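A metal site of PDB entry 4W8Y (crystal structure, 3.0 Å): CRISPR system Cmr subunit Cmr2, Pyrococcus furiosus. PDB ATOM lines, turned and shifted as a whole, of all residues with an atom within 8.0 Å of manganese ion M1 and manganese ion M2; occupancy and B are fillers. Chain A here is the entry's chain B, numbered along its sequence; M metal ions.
Manganese ion M1 is bound by OD2 of Asp 31 (2.1 Å), NE2 of His 30 (2.2 Å) and NE2 of His 224 (2.2 Å).
Manganese ion M1 has three donor atoms within binding distance.
Within 4 Å of manganese ion M2: Asp 31, Lys 35 and His 42.
Along chain A the residues within 4 Å of manganese ion M2 span positions 31 to 42.
Manganese ion M2 is bound by the side-chain carboxylate of Asp 31 (2.1 Å) and a ring nitrogen (NE2) of His 42 (2.3 Å).
Manganese ion M2 has two donor atoms within binding distance.
Slightly farther from manganese ion M2 lies the side-chain amino group (NZ) of Lys 35 (2.8 Å).
Of the 19 residues printed, 4 come within 4 Å of manganese ion M1.
A ring nitrogen (ND1) of His 42 sits at hydrogen-bond distance from the side-chain carboxylate of Glu 43 (3.4 Å).
The side-chain amino group of Lys 35 sits close to the side-chain carboxylate of Asp 31.
The backbone carbonyl oxygen (O) of His 30 sits at hydrogen-bond distance from the side-chain hydroxyl (OG) of Ser 46, at 3.2 Å.
A ring nitrogen (ND1) of His 42 sits at hydrogen-bond distance from the backbone carbonyl oxygen of Ile 39.
The backbone carbonyl oxygen (O) of His 224 is in hydrogen-bond range of the side-chain hydroxyl (OG1) of Thr 228, 2.6 Å away.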
ATOM      1  N   VAL A  27      -0.349 -30.359  28.186  1.00  0.00           N
ATOM      2  CA  VAL A  27      -1.704 -30.851  28.446  1.00  0.00           C
ATOM      3  C   VAL A  27      -2.335 -30.129  29.626  1.00  0.00           C
ATOM      4  O   VAL A  27      -3.556 -29.934  29.668  1.00  0.00           O
ATOM      5  CB  VAL A  27      -1.728 -32.380  28.688  1.00  0.00           C
ATOM      6  CG1 VAL A  27      -1.306 -33.122  27.431  1.00  0.00           C
ATOM      7  CG2 VAL A  27      -0.844 -32.770  29.869  1.00  0.00           C
ATOM      8  N   TYR A  28      -1.514 -29.734  30.596  1.00  0.00           N
ATOM      9  CA  TYR A  28      -2.006 -28.981  31.739  1.00  0.00           C
ATOM     10  C   TYR A  28      -2.460 -27.598  31.300  1.00  0.00           C
ATOM     11  O   TYR A  28      -3.570 -27.182  31.605  1.00  0.00           O
ATOM     12  CB  TYR A  28      -0.935 -28.861  32.826  1.00  0.00           C
ATOM     13  CG  TYR A  28      -1.454 -28.268  34.113  1.00  0.00           C
ATOM     14  CD1 TYR A  28      -2.266 -29.001  34.963  1.00  0.00           C
ATOM     15  CD2 TYR A  28      -1.125 -26.963  34.481  1.00  0.00           C
ATOM     16  CE1 TYR A  28      -2.746 -28.472  36.134  1.00  0.00           C
ATOM     17  CE2 TYR A  28      -1.608 -26.417  35.665  1.00  0.00           C
ATOM     18  CZ  TYR A  28      -2.420 -27.175  36.481  1.00  0.00           C
ATOM     19  OH  TYR A  28      -2.898 -26.640  37.659  1.00  0.00           O
ATOM     20  N   HIS A  30      -3.336 -26.578  28.430  1.00  0.00           N
ATOM     21  CA  HIS A  30      -4.143 -26.576  27.216  1.00  0.00           C
ATOM     22  C   HIS A  30      -5.072 -25.358  27.225  1.00  0.00           C
ATOM     23  O   HIS A  30      -5.335 -24.761  26.189  1.00  0.00           O
ATOM     24  CB  HIS A  30      -4.955 -27.873  27.081  1.00  0.00           C
ATOM     25  CG  HIS A  30      -6.284 -27.831  27.762  1.00  0.00           C
ATOM     26  ND1 HIS A  30      -6.415 -27.827  29.136  1.00  0.00           N
ATOM     27  CD2 HIS A  30      -7.539 -27.786  27.267  1.00  0.00           C
ATOM     28  CE1 HIS A  30      -7.701 -27.789  29.456  1.00  0.00           C
ATOM     29  NE2 HIS A  30      -8.402 -27.770  28.341  1.00  0.00           N
ATOM     30  N   ASP A  31      -5.580 -25.021  28.407  1.00  0.00           N
ATOM     31  CA  ASP A  31      -6.343 -23.794  28.614  1.00  0.00           C
ATOM     32  C   ASP A  31      -5.576 -22.854  29.551  1.00  0.00           C
ATOM     33  O   ASP A  31      -4.855 -23.300  30.430  1.00  0.00           O
ATOM     34  CB  ASP A  31      -7.729 -24.102  29.196  1.00  0.00           C
ATOM     35  CG  ASP A  31      -8.684 -24.640  28.150  1.00  0.00           C
ATOM     36  OD1 ASP A  31      -8.615 -24.191  26.989  1.00  0.00           O
ATOM     37  OD2 ASP A  31      -9.530 -25.497  28.497  1.00  0.00           O
ATOM     38  N   PRO A  32      -5.737 -21.539  29.343  1.00  0.00           N
ATOM     39  CA  PRO A  32      -5.032 -20.552  30.156  1.00  0.00           C
ATOM     40  C   PRO A  32      -5.758 -20.241  31.467  1.00  0.00           C
ATOM     41  O   PRO A  32      -6.972 -20.481  31.556  1.00  0.00           O
ATOM     42  CB  PRO A  32      -5.010 -19.320  29.259  1.00  0.00           C
ATOM     43  CG  PRO A  32      -6.276 -19.429  28.476  1.00  0.00           C
ATOM     44  CD  PRO A  32      -6.527 -20.904  28.275  1.00  0.00           C
ATOM     45  N   LYS A  35      -8.821 -17.855  31.137  1.00  0.00           N
ATOM     46  CA  LYS A  35      -9.808 -18.272  30.147  1.00  0.00           C
ATOM     47  C   LYS A  35     -11.094 -17.453  30.306  1.00  0.00           C
ATOM     48  O   LYS A  35     -11.819 -17.223  29.348  1.00  0.00           O
ATOM     49  CB  LYS A  35     -10.094 -19.774  30.273  1.00  0.00           C
ATOM     50  CG  LYS A  35     -11.183 -20.302  29.353  1.00  0.00           C
ATOM     51  CD  LYS A  35     -11.197 -21.826  29.360  1.00  0.00           C
ATOM     52  CE  LYS A  35     -12.274 -22.399  28.450  1.00  0.00           C
ATOM     53  NZ  LYS A  35     -12.005 -23.825  28.091  1.00  0.00           N
ATOM     54  N   ILE A  39     -13.056 -15.514  26.039  1.00  0.00           N
ATOM     55  CA  ILE A  39     -13.016 -16.909  25.621  1.00  0.00           C
ATOM     56  C   ILE A  39     -12.599 -17.021  24.148  1.00  0.00           C
ATOM     57  O   ILE A  39     -12.006 -18.019  23.728  1.00  0.00           O
ATOM     58  CB  ILE A  39     -14.376 -17.598  25.843  1.00  0.00           C
ATOM     59  CG1 ILE A  39     -14.807 -17.449  27.299  1.00  0.00           C
ATOM     60  CG2 ILE A  39     -14.316 -19.065  25.458  1.00  0.00           C
ATOM     61  CD1 ILE A  39     -15.997 -18.323  27.690  1.00  0.00           C
ATOM     62  N   HIS A  42      -8.686 -17.991  23.204  1.00  0.00           N
ATOM     63  CA  HIS A  42      -7.918 -18.276  24.407  1.00  0.00           C
ATOM     64  C   HIS A  42      -6.714 -19.182  24.075  1.00  0.00           C
ATOM     65  O   HIS A  42      -5.619 -19.050  24.644  1.00  0.00           O
ATOM     66  CB  HIS A  42      -8.807 -18.902  25.484  1.00  0.00           C
ATOM     67  CG  HIS A  42      -9.276 -20.285  25.156  1.00  0.00           C
ATOM     68  ND1 HIS A  42     -10.454 -20.548  24.489  1.00  0.00           N
ATOM     69  CD2 HIS A  42      -8.752 -21.488  25.485  1.00  0.00           C
ATOM     70  CE1 HIS A  42     -10.612 -21.851  24.383  1.00  0.00           C
ATOM     71  NE2 HIS A  42      -9.600 -22.450  24.982  1.00  0.00           N
ATOM     72  N   GLU A  43      -6.928 -20.089  23.117  1.00  0.00           N
ATOM     73  CA  GLU A  43      -5.888 -21.038  22.710  1.00  0.00           C
ATOM     74  C   GLU A  43      -4.622 -20.305  22.307  1.00  0.00           C
ATOM     75  O   GLU A  43      -3.528 -20.809  22.532  1.00  0.00           O
ATOM     76  CB  GLU A  43      -6.330 -21.924  21.537  1.00  0.00           C
ATOM     77  CG  GLU A  43      -7.567 -22.767  21.783  1.00  0.00           C
ATOM     78  CD  GLU A  43      -8.859 -22.007  21.585  1.00  0.00           C
ATOM     79  OE1 GLU A  43      -9.922 -22.657  21.480  1.00  0.00           O
ATOM     80  OE2 GLU A  43      -8.813 -20.760  21.559  1.00  0.00           O
ATOM     81  N   SER A  46      -2.744 -19.530  25.304  1.00  0.00           N
ATOM     82  CA  SER A  46      -2.100 -20.753  25.762  1.00  0.00           C
ATOM     83  C   SER A  46      -0.851 -21.055  24.948  1.00  0.00           C
ATOM     84  O   SER A  46       0.161 -21.500  25.481  1.00  0.00           O
ATOM     85  CB  SER A  46      -3.079 -21.933  25.676  1.00  0.00           C
ATOM     86  OG  SER A  46      -3.920 -21.979  26.817  1.00  0.00           O
ATOM     87  N   VAL A  63      -5.478 -34.441  25.049  1.00  0.00           N
ATOM     88  CA  VAL A  63      -6.384 -33.378  25.442  1.00  0.00           C
ATOM     89  C   VAL A  63      -7.768 -33.645  24.860  1.00  0.00           C
ATOM     90  O   VAL A  63      -8.780 -33.307  25.453  1.00  0.00           O
ATOM     91  CB  VAL A  63      -5.885 -31.985  24.984  1.00  0.00           C
ATOM     92  CG1 VAL A  63      -6.766 -30.884  25.552  1.00  0.00           C
ATOM     93  CG2 VAL A  63      -4.441 -31.788  25.415  1.00  0.00           C
ATOM     94  N   ALA A  66      -9.355 -36.363  27.061  1.00  0.00           N
ATOM     95  CA  ALA A  66      -9.713 -35.717  28.311  1.00  0.00           C
ATOM     96  C   ALA A  66     -10.977 -34.873  28.150  1.00  0.00           C
ATOM     97  O   ALA A  66     -11.885 -34.920  28.979  1.00  0.00           O
ATOM     98  CB  ALA A  66      -8.563 -34.865  28.814  1.00  0.00           C
ATOM     99  N   ASP A  67     -11.032 -34.105  27.068  1.00  0.00           N
ATOM    100  CA  ASP A  67     -12.164 -33.230  26.786  1.00  0.00           C
ATOM    101  C   ASP A  67     -13.443 -34.015  26.469  1.00  0.00           C
ATOM    102  O   ASP A  67     -14.532 -33.575  26.829  1.00  0.00           O
ATOM    103  CB  ASP A  67     -11.848 -32.279  25.631  1.00  0.00           C
ATOM    104  CG  ASP A  67     -10.868 -31.191  26.020  1.00  0.00           C
ATOM    105  OD1 ASP A  67     -10.319 -31.269  27.146  1.00  0.00           O
ATOM    106  OD2 ASP A  67     -10.647 -30.274  25.214  1.00  0.00           O
ATOM    107  N   SER A  70     -14.604 -35.570  29.720  1.00  0.00           N
ATOM    108  CA  SER A  70     -15.203 -34.472  30.473  1.00  0.00           C
ATOM    109  C   SER A  70     -16.585 -34.145  29.918  1.00  0.00           C
ATOM    110  O   SER A  70     -17.518 -33.838  30.670  1.00  0.00           O
ATOM    111  CB  SER A  70     -14.307 -33.242  30.443  1.00  0.00           C
ATOM    112  OG  SER A  70     -14.790 -32.218  31.294  1.00  0.00           O
ATOM    113  N   ALA A 212     -13.547 -21.749  35.569  1.00  0.00           N
ATOM    114  CA  ALA A 212     -13.101 -22.527  34.428  1.00  0.00           C
ATOM    115  C   ALA A 212     -14.142 -22.450  33.322  1.00  0.00           C
ATOM    116  O   ALA A 212     -13.814 -22.271  32.150  1.00  0.00           O
ATOM    117  CB  ALA A 212     -12.862 -23.964  34.827  1.00  0.00           C
ATOM    118  N   ILE A 221     -10.488 -22.333  37.611  1.00  0.00           N
ATOM    119  CA  ILE A 221      -9.838 -22.813  36.402  1.00  0.00           C
ATOM    120  C   ILE A 221      -8.815 -23.908  36.719  1.00  0.00           C
ATOM    121  O   ILE A 221      -8.660 -24.890  35.964  1.00  0.00           O
ATOM    122  CB  ILE A 221      -9.145 -21.636  35.652  1.00  0.00           C
ATOM    123  CG1 ILE A 221      -8.459 -22.138  34.374  1.00  0.00           C
ATOM    124  CG2 ILE A 221      -8.170 -20.886  36.565  1.00  0.00           C
ATOM    125  CD1 ILE A 221      -9.430 -22.553  33.284  1.00  0.00           C
ATOM    126  N   HIS A 224     -10.006 -27.521  36.858  1.00  0.00           N
ATOM    127  CA  HIS A 224     -10.268 -27.985  35.504  1.00  0.00           C
ATOM    128  C   HIS A 224      -8.979 -28.402  34.817  1.00  0.00           C
ATOM    129  O   HIS A 224      -8.934 -29.421  34.121  1.00  0.00           O
ATOM    130  CB  HIS A 224     -10.964 -26.916  34.686  1.00  0.00           C
ATOM    131  CG  HIS A 224     -11.186 -27.303  33.250  1.00  0.00           C
ATOM    132  ND1 HIS A 224     -11.746 -28.509  32.889  1.00  0.00           N
ATOM    133  CD2 HIS A 224     -10.914 -26.645  32.098  1.00  0.00           C
ATOM    134  CE1 HIS A 224     -11.814 -28.577  31.569  1.00  0.00           C
ATOM    135  NE2 HIS A 224     -11.317 -27.463  31.063  1.00  0.00           N
ATOM    136  N   LEU A 225      -7.941 -27.592  35.011  1.00  0.00           N
ATOM    137  CA  LEU A 225      -6.627 -27.927  34.454  1.00  0.00           C
ATOM    138  C   LEU A 225      -6.121 -29.239  35.053  1.00  0.00           C
ATOM    139  O   LEU A 225      -5.627 -30.118  34.335  1.00  0.00           O
ATOM    140  CB  LEU A 225      -5.634 -26.798  34.721  1.00  0.00           C
ATOM    141  CG  LEU A 225      -5.535 -25.643  33.716  1.00  0.00           C
ATOM    142  CD1 LEU A 225      -6.889 -25.236  33.171  1.00  0.00           C
ATOM    143  CD2 LEU A 225      -4.838 -24.457  34.361  1.00  0.00           C
ATOM    144  N   THR A 228      -8.094 -32.186  33.654  1.00  0.00           N
ATOM    145  CA  THR A 228      -7.744 -32.450  32.261  1.00  0.00           C
ATOM    146  C   THR A 228      -6.433 -33.236  32.192  1.00  0.00           C
ATOM    147  O   THR A 228      -6.329 -34.290  31.534  1.00  0.00           O
ATOM    148  CB  THR A 228      -7.594 -31.134  31.459  1.00  0.00           C
ATOM    149  OG1 THR A 228      -8.748 -30.316  31.647  1.00  0.00           O
ATOM    150  CG2 THR A 228      -7.422 -31.426  29.968  1.00  0.00           C
HETATM  151 MN    MN M   1     -10.469 -27.349  28.997  1.00  0.00          MN
HETATM  152 MN    MN M   2     -10.390 -24.387  25.813  1.00  0.00          MN
